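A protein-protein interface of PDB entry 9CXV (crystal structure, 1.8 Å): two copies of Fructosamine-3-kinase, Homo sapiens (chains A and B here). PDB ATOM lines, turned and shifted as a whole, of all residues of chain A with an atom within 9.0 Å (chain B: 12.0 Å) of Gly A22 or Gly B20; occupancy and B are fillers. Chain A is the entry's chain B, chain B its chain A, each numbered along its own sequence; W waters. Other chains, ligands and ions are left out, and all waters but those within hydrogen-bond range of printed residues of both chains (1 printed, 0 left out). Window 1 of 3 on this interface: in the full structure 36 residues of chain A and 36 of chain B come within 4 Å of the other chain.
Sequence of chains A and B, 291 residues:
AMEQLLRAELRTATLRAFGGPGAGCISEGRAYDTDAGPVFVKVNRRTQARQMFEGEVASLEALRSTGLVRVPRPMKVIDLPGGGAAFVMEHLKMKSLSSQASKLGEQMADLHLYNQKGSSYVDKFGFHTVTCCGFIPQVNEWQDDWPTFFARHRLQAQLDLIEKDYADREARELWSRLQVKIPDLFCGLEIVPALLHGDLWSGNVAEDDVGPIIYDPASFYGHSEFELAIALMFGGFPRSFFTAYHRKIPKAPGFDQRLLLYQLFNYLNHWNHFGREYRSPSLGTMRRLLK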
ATOM      1  N   GLY A  19      -9.509  -6.092  32.470  1.00  0.00           N
ATOM      2  CA  GLY A  19      -9.822  -4.717  32.119  1.00  0.00           C
ATOM      3  C   GLY A  19     -11.290  -4.345  32.275  1.00  0.00           C
ATOM      4  O   GLY A  19     -11.666  -3.174  32.123  1.00  0.00           O
ATOM      5  N   GLY A  22      -7.957   5.036  30.765  1.00  0.00           N
ATOM      6  CA  GLY A  22      -9.383   5.332  30.735  1.00  0.00           C
ATOM      7  C   GLY A  22     -10.208   4.112  30.358  1.00  0.00           C
ATOM      8  O   GLY A  22      -9.782   3.319  29.514  1.00  0.00           O
ATOM      9  N   ALA A  23     -11.388   3.959  30.973  1.00  0.00           N
ATOM     10  CA  ALA A  23     -12.242   2.787  30.789  1.00  0.00           C
ATOM     11  C   ALA A  23     -13.708   3.202  30.870  1.00  0.00           C
ATOM     12  O   ALA A  23     -14.063   4.142  31.586  1.00  0.00           O
ATOM     13  CB  ALA A  23     -11.950   1.699  31.843  1.00  0.00           C
ATOM     14  N   GLY A  24     -14.562   2.503  30.129  1.00  0.00           N
ATOM     15  CA  GLY A  24     -15.991   2.751  30.229  1.00  0.00           C
ATOM     16  C   GLY A  24     -16.703   3.061  28.922  1.00  0.00           C
ATOM     17  O   GLY A  24     -16.115   3.587  27.972  1.00  0.00           O
ATOM     18  N   CYS A  25     -18.004   2.749  28.883  1.00  0.00           N
ATOM     19  CA  CYS A  25     -18.844   2.940  27.704  1.00  0.00           C
ATOM     20  C   CYS A  25     -19.483   4.314  27.647  1.00  0.00           C
ATOM     21  O   CYS A  25     -19.833   4.784  26.562  1.00  0.00           O
ATOM     22  CB  CYS A  25     -19.949   1.867  27.676  1.00  0.00           C
ATOM     23  SG  CYS A  25     -19.284   0.191  27.633  1.00  0.00           S
ATOM     24  N   SER A  27     -18.650   7.054  30.313  1.00  0.00           N
ATOM     25  CA  SER A  27     -17.778   8.043  30.904  1.00  0.00           C
ATOM     26  C   SER A  27     -16.342   7.574  30.763  1.00  0.00           C
ATOM     27  O   SER A  27     -16.072   6.394  30.532  1.00  0.00           O
ATOM     28  CB  SER A  27     -18.108   8.242  32.393  1.00  0.00           C
ATOM     29  OG  SER A  27     -19.463   8.650  32.538  1.00  0.00           O
ATOM     30  N   GLU A  28     -15.430   8.509  30.978  1.00  0.00           N
ATOM     31  CA  GLU A  28     -14.003   8.214  31.097  1.00  0.00           C
ATOM     32  C   GLU A  28     -13.685   7.946  32.568  1.00  0.00           C
ATOM     33  O   GLU A  28     -13.878   8.832  33.395  1.00  0.00           O
ATOM     34  CB  GLU A  28     -13.214   9.429  30.622  1.00  0.00           C
ATOM     35  CG  GLU A  28     -11.788   9.148  30.247  1.00  0.00           C
ATOM     36  CD  GLU A  28     -11.061  10.434  29.913  1.00  0.00           C
ATOM     37  OE1 GLU A  28     -11.733  11.337  29.364  1.00  0.00           O
ATOM     38  OE2 GLU A  28      -9.838  10.528  30.185  1.00  0.00           O
ATOM     39  N   GLY A  29     -13.140   6.791  32.890  1.00  0.00           N
ATOM     40  CA  GLY A  29     -12.889   6.416  34.282  1.00  0.00           C
ATOM     41  C   GLY A  29     -11.421   6.150  34.540  1.00  0.00           C
ATOM     42  O   GLY A  29     -10.783   5.437  33.780  1.00  0.00           O
ATOM     43  N   ARG A  30     -10.894   6.703  35.636  1.00  0.00           N
ATOM     44  CA  ARG A  30      -9.474   6.521  35.951  1.00  0.00           C
ATOM     45  C   ARG A  30      -9.238   6.450  37.448  1.00  0.00           C
ATOM     46  O   ARG A  30      -9.907   7.116  38.225  1.00  0.00           O
ATOM     47  CB  ARG A  30      -8.594   7.643  35.398  1.00  0.00           C
ATOM     48  CG  ARG A  30      -9.061   8.218  34.057  1.00  0.00           C
ATOM     49  CD  ARG A  30      -8.609   9.656  33.893  1.00  0.00           C
ATOM     50  NE  ARG A  30      -7.178   9.692  33.626  1.00  0.00           N
ATOM     51  CZ  ARG A  30      -6.621   9.474  32.444  1.00  0.00           C
ATOM     52  NH1 ARG A  30      -7.356   9.213  31.369  1.00  0.00           N
ATOM     53  NH2 ARG A  30      -5.292   9.522  32.341  1.00  0.00           N
ATOM     54  N   ALA A  31      -8.258   5.651  37.840  1.00  0.00           N
ATOM     55  CA  ALA A  31      -7.899   5.529  39.235  1.00  0.00           C
ATOM     56  C   ALA A  31      -6.746   6.465  39.554  1.00  0.00           C
ATOM     57  O   ALA A  31      -5.805   6.609  38.757  1.00  0.00           O
ATOM     58  CB  ALA A  31      -7.481   4.102  39.563  1.00  0.00           C
ATOM     59  N   TYR A  32      -6.816   7.074  40.730  1.00  0.00           N
ATOM     60  CA  TYR A  32      -5.758   7.942  41.229  1.00  0.00           C
ATOM     61  C   TYR A  32      -5.377   7.538  42.640  1.00  0.00           C
ATOM     62  O   TYR A  32      -6.247   7.282  43.489  1.00  0.00           O
ATOM     63  CB  TYR A  32      -6.212   9.389  41.287  1.00  0.00           C
ATOM     64  CG  TYR A  32      -6.499   9.996  39.969  1.00  0.00           C
ATOM     65  CD1 TYR A  32      -5.468  10.488  39.162  1.00  0.00           C
ATOM     66  CD2 TYR A  32      -7.815  10.071  39.508  1.00  0.00           C
ATOM     67  CE1 TYR A  32      -5.742  11.091  37.937  1.00  0.00           C
ATOM     68  CE2 TYR A  32      -8.108  10.666  38.302  1.00  0.00           C
ATOM     69  CZ  TYR A  32      -7.058  11.178  37.520  1.00  0.00           C
ATOM     70  OH  TYR A  32      -7.354  11.722  36.326  1.00  0.00           O
ATOM     71  N   PHE A  40     -11.446   6.244  42.499  1.00  0.00           N
ATOM     72  CA  PHE A  40     -11.794   6.052  41.100  1.00  0.00           C
ATOM     73  C   PHE A  40     -12.680   7.200  40.668  1.00  0.00           C
ATOM     74  O   PHE A  40     -13.601   7.589  41.380  1.00  0.00           O
ATOM     75  CB  PHE A  40     -12.501   4.711  40.874  1.00  0.00           C
ATOM     76  CG  PHE A  40     -12.685   4.386  39.441  1.00  0.00           C
ATOM     77  CD1 PHE A  40     -11.620   3.902  38.685  1.00  0.00           C
ATOM     78  CD2 PHE A  40     -13.946   4.568  38.830  1.00  0.00           C
ATOM     79  CE1 PHE A  40     -11.803   3.612  37.326  1.00  0.00           C
ATOM     80  CE2 PHE A  40     -14.143   4.250  37.472  1.00  0.00           C
ATOM     81  CZ  PHE A  40     -13.059   3.779  36.729  1.00  0.00           C
ATOM     82  N   VAL A  41     -12.383   7.787  39.521  1.00  0.00           N
ATOM     83  CA  VAL A  41     -13.067   8.992  39.087  1.00  0.00           C
ATOM     84  C   VAL A  41     -13.634   8.740  37.697  1.00  0.00           C
ATOM     85  O   VAL A  41     -12.901   8.327  36.802  1.00  0.00           O
ATOM     86  CB  VAL A  41     -12.096  10.192  39.058  1.00  0.00           C
ATOM     87  CG1 VAL A  41     -12.853  11.444  38.617  1.00  0.00           C
ATOM     88  CG2 VAL A  41     -11.490  10.387  40.463  1.00  0.00           C
ATOM     89  N   HIS A  91     -12.062   3.414  45.461  1.00  0.00           N
ATOM     90  CA  HIS A  91     -11.395   2.550  44.500  1.00  0.00           C
ATOM     91  C   HIS A  91     -11.405   1.142  45.040  1.00  0.00           C
ATOM     92  O   HIS A  91     -11.137   0.930  46.231  1.00  0.00           O
ATOM     93  CB  HIS A  91      -9.932   2.974  44.291  1.00  0.00           C
ATOM     94  CG  HIS A  91      -9.193   2.090  43.340  1.00  0.00           C
ATOM     95  ND1 HIS A  91      -8.495   0.971  43.753  1.00  0.00           N
ATOM     96  CD2 HIS A  91      -9.068   2.139  41.995  1.00  0.00           C
ATOM     97  CE1 HIS A  91      -7.973   0.361  42.694  1.00  0.00           C
ATOM     98  NE2 HIS A  91      -8.288   1.057  41.618  1.00  0.00           N
ATOM     99  N   MET B   2      -8.771  19.617  35.089  1.00  0.00           N
ATOM    100  CA  MET B   2      -9.633  18.748  35.876  1.00  0.00           C
ATOM    101  C   MET B   2      -8.834  18.079  37.007  1.00  0.00           C
ATOM    102  O   MET B   2      -9.354  17.945  38.126  1.00  0.00           O
ATOM    103  CB  MET B   2     -10.356  17.782  34.917  1.00  0.00           C
ATOM    104  CG  MET B   2     -11.488  16.866  35.489  1.00  0.00           C
ATOM    105  SD  MET B   2     -10.701  15.426  36.194  1.00  0.00           S
ATOM    106  CE  MET B   2      -9.791  14.737  34.802  1.00  0.00           C
ATOM    107  N   GLU B   3      -7.538  17.784  36.789  1.00  0.00           N
ATOM    108  CA  GLU B   3      -6.696  17.203  37.847  1.00  0.00           C
ATOM    109  C   GLU B   3      -6.456  18.179  39.008  1.00  0.00           C
ATOM    110  O   GLU B   3      -6.379  17.762  40.170  1.00  0.00           O
ATOM    111  CB  GLU B   3      -5.340  16.762  37.288  1.00  0.00           C
ATOM    112  CG  GLU B   3      -5.394  15.909  36.031  1.00  0.00           C
ATOM    113  CD  GLU B   3      -4.610  14.601  36.134  1.00  0.00           C
ATOM    114  OE1 GLU B   3      -5.120  13.594  35.568  1.00  0.00           O
ATOM    115  OE2 GLU B   3      -3.515  14.572  36.774  1.00  0.00           O
ATOM    116  N   LEU B  15      -1.868  13.016  43.413  1.00  0.00           N
ATOM    117  CA  LEU B  15      -2.961  12.562  42.577  1.00  0.00           C
ATOM    118  C   LEU B  15      -2.314  11.839  41.408  1.00  0.00           C
ATOM    119  O   LEU B  15      -2.212  12.399  40.309  1.00  0.00           O
ATOM    120  CB  LEU B  15      -3.827  13.731  42.089  1.00  0.00           C
ATOM    121  CG  LEU B  15      -5.121  13.295  41.388  1.00  0.00           C
ATOM    122  CD1 LEU B  15      -6.264  13.160  42.419  1.00  0.00           C
ATOM    123  CD2 LEU B  15      -5.478  14.200  40.228  1.00  0.00           C
ATOM    124  N   ARG B  16      -1.827  10.623  41.645  1.00  0.00           N
ATOM    125  CA  ARG B  16      -1.001   9.912  40.674  1.00  0.00           C
ATOM    126  C   ARG B  16      -1.866   8.876  39.987  1.00  0.00           C
ATOM    127  O   ARG B  16      -2.309   7.913  40.622  1.00  0.00           O
ATOM    128  CB  ARG B  16       0.210   9.253  41.344  1.00  0.00           C
ATOM    129  N   ALA B  17      -2.099   9.064  38.697  1.00  0.00           N
ATOM    130  CA  ALA B  17      -2.835   8.069  37.930  1.00  0.00           C
ATOM    131  C   ALA B  17      -2.173   6.695  38.058  1.00  0.00           C
ATOM    132  O   ALA B  17      -0.975   6.575  38.330  1.00  0.00           O
ATOM    133  CB  ALA B  17      -2.935   8.515  36.465  1.00  0.00           C
ATOM    134  N   PHE B  18      -2.982   5.648  37.918  1.00  0.00           N
ATOM    135  CA  PHE B  18      -2.497   4.270  37.902  1.00  0.00           C
ATOM    136  C   PHE B  18      -3.606   3.404  37.323  1.00  0.00           C
ATOM    137  O   PHE B  18      -4.705   3.888  37.047  1.00  0.00           O
ATOM    138  CB  PHE B  18      -2.059   3.795  39.293  1.00  0.00           C
ATOM    139  CG  PHE B  18      -3.202   3.455  40.254  1.00  0.00           C
ATOM    140  CD1 PHE B  18      -3.719   2.148  40.322  1.00  0.00           C
ATOM    141  CD2 PHE B  18      -3.701   4.408  41.143  1.00  0.00           C
ATOM    142  CE1 PHE B  18      -4.735   1.809  41.247  1.00  0.00           C
ATOM    143  CE2 PHE B  18      -4.741   4.068  42.069  1.00  0.00           C
ATOM    144  CZ  PHE B  18      -5.237   2.762  42.101  1.00  0.00           C
ATOM    145  N   GLY B  19      -3.306   2.121  37.118  1.00  0.00           N
ATOM    146  CA  GLY B  19      -4.285   1.207  36.551  1.00  0.00           C
ATOM    147  C   GLY B  19      -4.646   1.470  35.106  1.00  0.00           C
ATOM    148  O   GLY B  19      -5.538   0.789  34.576  1.00  0.00           O
ATOM    149  N   GLY B  20      -3.998   2.450  34.467  1.00  0.00           N
ATOM    150  CA  GLY B  20      -4.152   2.740  33.048  1.00  0.00           C
ATOM    151  C   GLY B  20      -5.562   2.959  32.545  1.00  0.00           C
ATOM    152  O   GLY B  20      -5.813   2.815  31.347  1.00  0.00           O
ATOM    153  N   CYS B  25     -16.742  -3.072  24.476  1.00  0.00           N
ATOM    154  CA  CYS B  25     -17.602  -1.905  24.681  1.00  0.00           C
ATOM    155  C   CYS B  25     -17.674  -0.940  23.481  1.00  0.00           C
ATOM    156  O   CYS B  25     -16.828  -0.985  22.576  1.00  0.00           O
ATOM    157  CB  CYS B  25     -17.147  -1.134  25.910  1.00  0.00           C
ATOM    158  SG  CYS B  25     -18.036   0.410  26.039  1.00  0.00           S
ATOM    159  N   ILE B  26     -18.666  -0.038  23.516  1.00  0.00           N
ATOM    160  CA  ILE B  26     -19.142   0.685  22.335  1.00  0.00           C
ATOM    161  C   ILE B  26     -19.557  -0.355  21.302  1.00  0.00           C
ATOM    162  O   ILE B  26     -19.406  -0.141  20.089  1.00  0.00           O
ATOM    163  CB  ILE B  26     -18.090   1.659  21.763  1.00  0.00           C
ATOM    164  N   GLY B  29     -16.391  -5.564  22.419  1.00  0.00           N
ATOM    165  CA  GLY B  29     -16.141  -6.879  22.974  1.00  0.00           C
ATOM    166  C   GLY B  29     -15.179  -6.762  24.128  1.00  0.00           C
ATOM    167  O   GLY B  29     -15.213  -5.757  24.838  1.00  0.00           O
ATOM    168  N   ALA B  31     -11.279  -8.341  26.237  1.00  0.00           N
ATOM    169  CA  ALA B  31      -9.915  -8.834  26.138  1.00  0.00           C
ATOM    170  C   ALA B  31      -9.724  -9.978  27.112  1.00  0.00           C
ATOM    171  O   ALA B  31     -10.373 -10.013  28.160  1.00  0.00           O
ATOM    172  CB  ALA B  31      -8.919  -7.733  26.468  1.00  0.00           C
ATOM    173  N   PHE B  40      -7.181  -9.766  22.076  1.00  0.00           N
ATOM    174  CA  PHE B  40      -8.337  -8.921  22.155  1.00  0.00           C
ATOM    175  C   PHE B  40      -9.386  -9.468  21.206  1.00  0.00           C
ATOM    176  O   PHE B  40      -9.086  -9.762  20.043  1.00  0.00           O
ATOM    177  CB  PHE B  40      -7.979  -7.452  21.851  1.00  0.00           C
ATOM    178  CG  PHE B  40      -9.121  -6.535  22.052  1.00  0.00           C
ATOM    179  CD1 PHE B  40      -9.376  -6.003  23.310  1.00  0.00           C
ATOM    180  CD2 PHE B  40      -9.976  -6.231  21.013  1.00  0.00           C
ATOM    181  CE1 PHE B  40     -10.468  -5.171  23.510  1.00  0.00           C
ATOM    182  CE2 PHE B  40     -11.055  -5.396  21.198  1.00  0.00           C
ATOM    183  CZ  PHE B  40     -11.312  -4.858  22.451  1.00  0.00           C
ATOM    184  N   HIS B  91      -3.251  -8.562  21.168  1.00  0.00           N
ATOM    185  CA  HIS B  91      -3.596  -7.544  22.140  1.00  0.00           C
ATOM    186  C   HIS B  91      -2.443  -6.561  22.274  1.00  0.00           C
ATOM    187  O   HIS B  91      -1.273  -6.958  22.263  1.00  0.00           O
ATOM    188  CB  HIS B  91      -3.892  -8.182  23.493  1.00  0.00           C
ATOM    189  CG  HIS B  91      -4.114  -7.189  24.579  1.00  0.00           C
ATOM    190  ND1 HIS B  91      -3.075  -6.619  25.291  1.00  0.00           N
ATOM    191  CD2 HIS B  91      -5.254  -6.617  25.042  1.00  0.00           C
ATOM    192  CE1 HIS B  91      -3.572  -5.769  26.177  1.00  0.00           C
ATOM    193  NE2 HIS B  91      -4.890  -5.752  26.050  1.00  0.00           N
ATOM    194  N   LEU B  92      -2.775  -5.283  22.403  1.00  0.00           N
ATOM    195  CA  LEU B  92      -1.773  -4.220  22.518  1.00  0.00           C
ATOM    196  C   LEU B  92      -2.085  -3.385  23.756  1.00  0.00           C
ATOM    197  O   LEU B  92      -3.208  -2.906  23.901  1.00  0.00           O
ATOM    198  CB  LEU B  92      -1.796  -3.314  21.268  1.00  0.00           C
ATOM    199  CG  LEU B  92      -1.300  -3.993  19.989  1.00  0.00           C
ATOM    200  CD1 LEU B  92      -1.573  -3.062  18.797  1.00  0.00           C
ATOM    201  CD2 LEU B  92       0.172  -4.392  20.067  1.00  0.00           C
ATOM    202  N   LYS B  93      -1.105  -3.204  24.649  1.00  0.00           N
ATOM    203  CA  LYS B  93      -1.327  -2.304  25.775  1.00  0.00           C
ATOM    204  C   LYS B  93      -1.264  -0.895  25.214  1.00  0.00           C
ATOM    205  O   LYS B  93      -0.263  -0.539  24.592  1.00  0.00           O
ATOM    206  CB  LYS B  93      -0.280  -2.526  26.868  1.00  0.00           C
ATOM    207  N   MET B  94      -2.347  -0.123  25.359  1.00  0.00           N
ATOM    208  CA  MET B  94      -2.475   1.166  24.677  1.00  0.00           C
ATOM    209  C   MET B  94      -2.901   2.280  25.631  1.00  0.00           C
ATOM    210  O   MET B  94      -3.623   2.049  26.611  1.00  0.00           O
ATOM    211  CB  MET B  94      -3.524   1.081  23.562  1.00  0.00           C
ATOM    212  CG  MET B  94      -3.164   0.215  22.392  1.00  0.00           C
ATOM    213  SD  MET B  94      -4.636   0.004  21.314  1.00  0.00           S
ATOM    214  CE  MET B  94      -5.890   0.757  22.280  1.00  0.00           C
ATOM    215  N   LYS B  95      -2.501   3.505  25.290  1.00  0.00           N
ATOM    216  CA  LYS B  95      -2.933   4.734  25.954  1.00  0.00           C
ATOM    217  C   LYS B  95      -3.239   5.771  24.881  1.00  0.00           C
ATOM    218  O   LYS B  95      -2.852   5.611  23.715  1.00  0.00           O
ATOM    219  CB  LYS B  95      -1.852   5.262  26.922  1.00  0.00           C
ATOM    220  N   SER B  96      -3.935   6.836  25.296  1.00  0.00           N
ATOM    221  CA  SER B  96      -4.342   7.930  24.413  1.00  0.00           C
ATOM    222  C   SER B  96      -3.150   8.472  23.636  1.00  0.00           C
ATOM    223  O   SER B  96      -2.053   8.602  24.186  1.00  0.00           O
ATOM    224  CB  SER B  96      -4.933   9.083  25.243  1.00  0.00           C
ATOM    225  OG  SER B  96      -6.304   8.858  25.471  1.00  0.00           O
ATOM    226  N   LEU B  97      -3.382   8.851  22.372  1.00  0.00           N
ATOM    227  CA  LEU B  97      -2.289   9.417  21.581  1.00  0.00           C
ATOM    228  C   LEU B  97      -1.885  10.755  22.167  1.00  0.00           C
ATOM    229  O   LEU B  97      -2.718  11.665  22.261  1.00  0.00           O
ATOM    230  CB  LEU B  97      -2.695   9.599  20.120  1.00  0.00           C
ATOM    231  CG  LEU B  97      -1.619  10.185  19.185  1.00  0.00           C
ATOM    232  CD1 LEU B  97      -0.434   9.222  18.929  1.00  0.00           C
ATOM    233  CD2 LEU B  97      -2.331  10.661  17.845  1.00  0.00           C
ATOM    234  N   SER B 202     -10.169  10.068  16.580  1.00  0.00           N
ATOM    235  CA  SER B 202      -9.215   9.994  17.677  1.00  0.00           C
ATOM    236  C   SER B 202      -9.419   8.710  18.468  1.00  0.00           C
ATOM    237  O   SER B 202      -8.491   8.230  19.137  1.00  0.00           O
ATOM    238  CB  SER B 202      -9.324  11.218  18.622  1.00  0.00           C
ATOM    239  OG  SER B 202     -10.670  11.337  19.093  1.00  0.00           O
ATOM    240  N   GLY B 203     -10.633   8.168  18.439  1.00  0.00           N
ATOM    241  CA  GLY B 203     -10.846   6.972  19.228  1.00  0.00           C
ATOM    242  C   GLY B 203     -10.313   5.709  18.587  1.00  0.00           C
ATOM    243  O   GLY B 203     -10.366   4.633  19.207  1.00  0.00           O
ATOM    244  N   VAL B 205      -7.039   5.665  17.396  1.00  0.00           N
ATOM    245  CA  VAL B 205      -5.585   5.795  17.425  1.00  0.00           C
ATOM    246  C   VAL B 205      -5.151   5.859  18.875  1.00  0.00           C
ATOM    247  O   VAL B 205      -5.929   6.246  19.743  1.00  0.00           O
ATOM    248  CB  VAL B 205      -5.055   7.041  16.672  1.00  0.00           C
ATOM    249  CG1 VAL B 205      -5.622   7.072  15.232  1.00  0.00           C
ATOM    250  CG2 VAL B 205      -5.479   8.361  17.406  1.00  0.00           C
ATOM    251  N   ALA B 206      -3.912   5.473  19.120  1.00  0.00           N
ATOM    252  CA  ALA B 206      -3.392   5.355  20.476  1.00  0.00           C
ATOM    253  C   ALA B 206      -1.878   5.262  20.417  1.00  0.00           C
ATOM    254  O   ALA B 206      -1.252   5.458  19.366  1.00  0.00           O
ATOM    255  CB  ALA B 206      -3.963   4.118  21.185  1.00  0.00           C
ATOM    256  N   GLU B 207      -1.268   4.907  21.548  1.00  0.00           N
ATOM    257  CA  GLU B 207       0.164   4.690  21.525  1.00  0.00           C
ATOM    258  C   GLU B 207       0.541   3.804  22.711  1.00  0.00           C
ATOM    259  O   GLU B 207      -0.238   3.629  23.653  1.00  0.00           O
ATOM    260  CB  GLU B 207       0.931   6.020  21.579  1.00  0.00           C
ATOM    261  CG  GLU B 207       0.789   6.706  22.993  1.00  0.00           C
ATOM    262  CD  GLU B 207       1.403   8.092  23.072  1.00  0.00           C
ATOM    263  OE1 GLU B 207       1.134   8.964  22.191  1.00  0.00           O
ATOM    264  OE2 GLU B 207       2.167   8.306  24.044  1.00  0.00           O
ATOM    265  N   ASP B 208       1.741   3.244  22.618  1.00  0.00           N
ATOM    266  CA  ASP B 208       2.415   2.605  23.753  1.00  0.00           C
ATOM    267  C   ASP B 208       3.804   3.229  23.921  1.00  0.00           C
ATOM    268  O   ASP B 208       4.101   4.331  23.441  1.00  0.00           O
ATOM    269  CB  ASP B 208       2.430   1.091  23.537  1.00  0.00           C
ATOM    270  CG  ASP B 208       3.236   0.659  22.301  1.00  0.00           C
ATOM    271  OD1 ASP B 208       4.081   1.421  21.782  1.00  0.00           O
ATOM    272  OD2 ASP B 208       2.986  -0.469  21.832  1.00  0.00           O
ATOM    273  N   ASP B 209       4.694   2.524  24.636  1.00  0.00           N
ATOM    274  CA  ASP B 209       6.044   3.034  24.851  1.00  0.00           C
ATOM    275  C   ASP B 209       6.906   2.994  23.590  1.00  0.00           C
ATOM    276  O   ASP B 209       7.905   3.728  23.518  1.00  0.00           O
ATOM    277  CB  ASP B 209       6.750   2.241  25.965  1.00  0.00           C
ATOM    278  CG  ASP B 209       6.171   2.509  27.337  1.00  0.00           C
ATOM    279  OD1 ASP B 209       5.346   3.451  27.461  1.00  0.00           O
ATOM    280  OD2 ASP B 209       6.566   1.793  28.296  1.00  0.00           O
ATOM    281  N   TYR B 215      -5.998   1.451  14.650  1.00  0.00           N
ATOM    282  CA  TYR B 215      -6.774   0.197  14.618  1.00  0.00           C
ATOM    283  C   TYR B 215      -8.190   0.520  14.148  1.00  0.00           C
ATOM    284  O   TYR B 215      -8.515   1.675  13.832  1.00  0.00           O
ATOM    285  CB  TYR B 215      -6.741  -0.478  16.023  1.00  0.00           C
ATOM    286  CG  TYR B 215      -7.143   0.467  17.145  1.00  0.00           C
ATOM    287  CD1 TYR B 215      -8.475   0.682  17.461  1.00  0.00           C
ATOM    288  CD2 TYR B 215      -6.163   1.157  17.871  1.00  0.00           C
ATOM    289  CE1 TYR B 215      -8.834   1.587  18.459  1.00  0.00           C
ATOM    290  CE2 TYR B 215      -6.513   2.063  18.865  1.00  0.00           C
ATOM    291  CZ  TYR B 215      -7.849   2.256  19.163  1.00  0.00           C
ATOM    292  OH  TYR B 215      -8.222   3.133  20.161  1.00  0.00           O
HETATM  293  O   HOH W   1      -6.937   4.005  35.624  1.00  0.00           O
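SG of Cys B25 forms a disulfide with SG of Cys A25 (2.0 Å).
The backbone NH (N) of Gly A22 sits at hydrogen-bond distance from the backbone carbonyl oxygen (O) of Gly B20, 3.1 Å away.
The side-chain carboxylate of Glu B3 is in hydrogen-bond range of the side-chain hydroxyl of Tyr A32 (3.0 Å).
N of Phe B18 lies within hydrogen-bond range of O of Ala A31 (3.1 Å).
The guanidinium group of Arg A30 is in hydrogen-bond range of the side-chain hydroxyl of Tyr A32, at 3.4 Å.
CA of Ala B17 touches O of Ala A31 (3.4 Å).
Tyr A32 touches Leu B15 (CD1 to CG, 3.6 Å).
Arg B16 touches Tyr A32 (O to CA, 3.5 Å).
CD1 of Tyr A32 touches N of Ala B17, 3.7 Å away.
CE2 of Phe B18 touches C of Tyr A32 (3.6 Å).
CZ of Phe B18 touches NE2 of His A91, 3.5 Å away.
Gly A22 touches just one residue of chain B: Gly B20 (3.1 Å).
Gly B20 touches just one residue of chain A: Gly A22.
No residue of chain B comes within 4 Å of Gly A29.
Arg A30 touches none of the printed residues of chain B.
No residue of chain A comes within 4 Å of Gly B19.
Printed residues of chain A within 4 Å of Cys B25: Cys A25 (2.0 Å).
Printed residues of chain A within 4 Å of Phe B18: Ala A31 (3.1 Å), Tyr A32 (3.6 Å) and His A91 (3.5 Å).
Of the printed residues of chain A, Arg B16 touches Tyr A32.
Of the printed residues of chain B, His A91 touches Phe B18 (3.5 Å).
The nearest residue of chain B that does not touch Gly A22 is Gly B19 (6.2 Å).
The nearest residue of chain A that does not touch Gly B20 is Ala A23 (5.7 Å).
The nearest printed residue of chain A that does not touch Phe B18 is Arg A30 (5.2 Å).
Hydrophobic or aromatic side chains of chain B that line the printed part of chain A: Leu B15 and Phe B18.
Hydrophobic or aromatic side chains of chain A within 4 Å of the printed part of chain B: Ala A31, Tyr A32 and His A91.
Cys A25 touches its own counterpart, Cys B25.
6 positions are printed for both chains.
Water W1 bridges O of Phe B18 (2.6 Å) and N of Ala A31 (3.1 Å).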
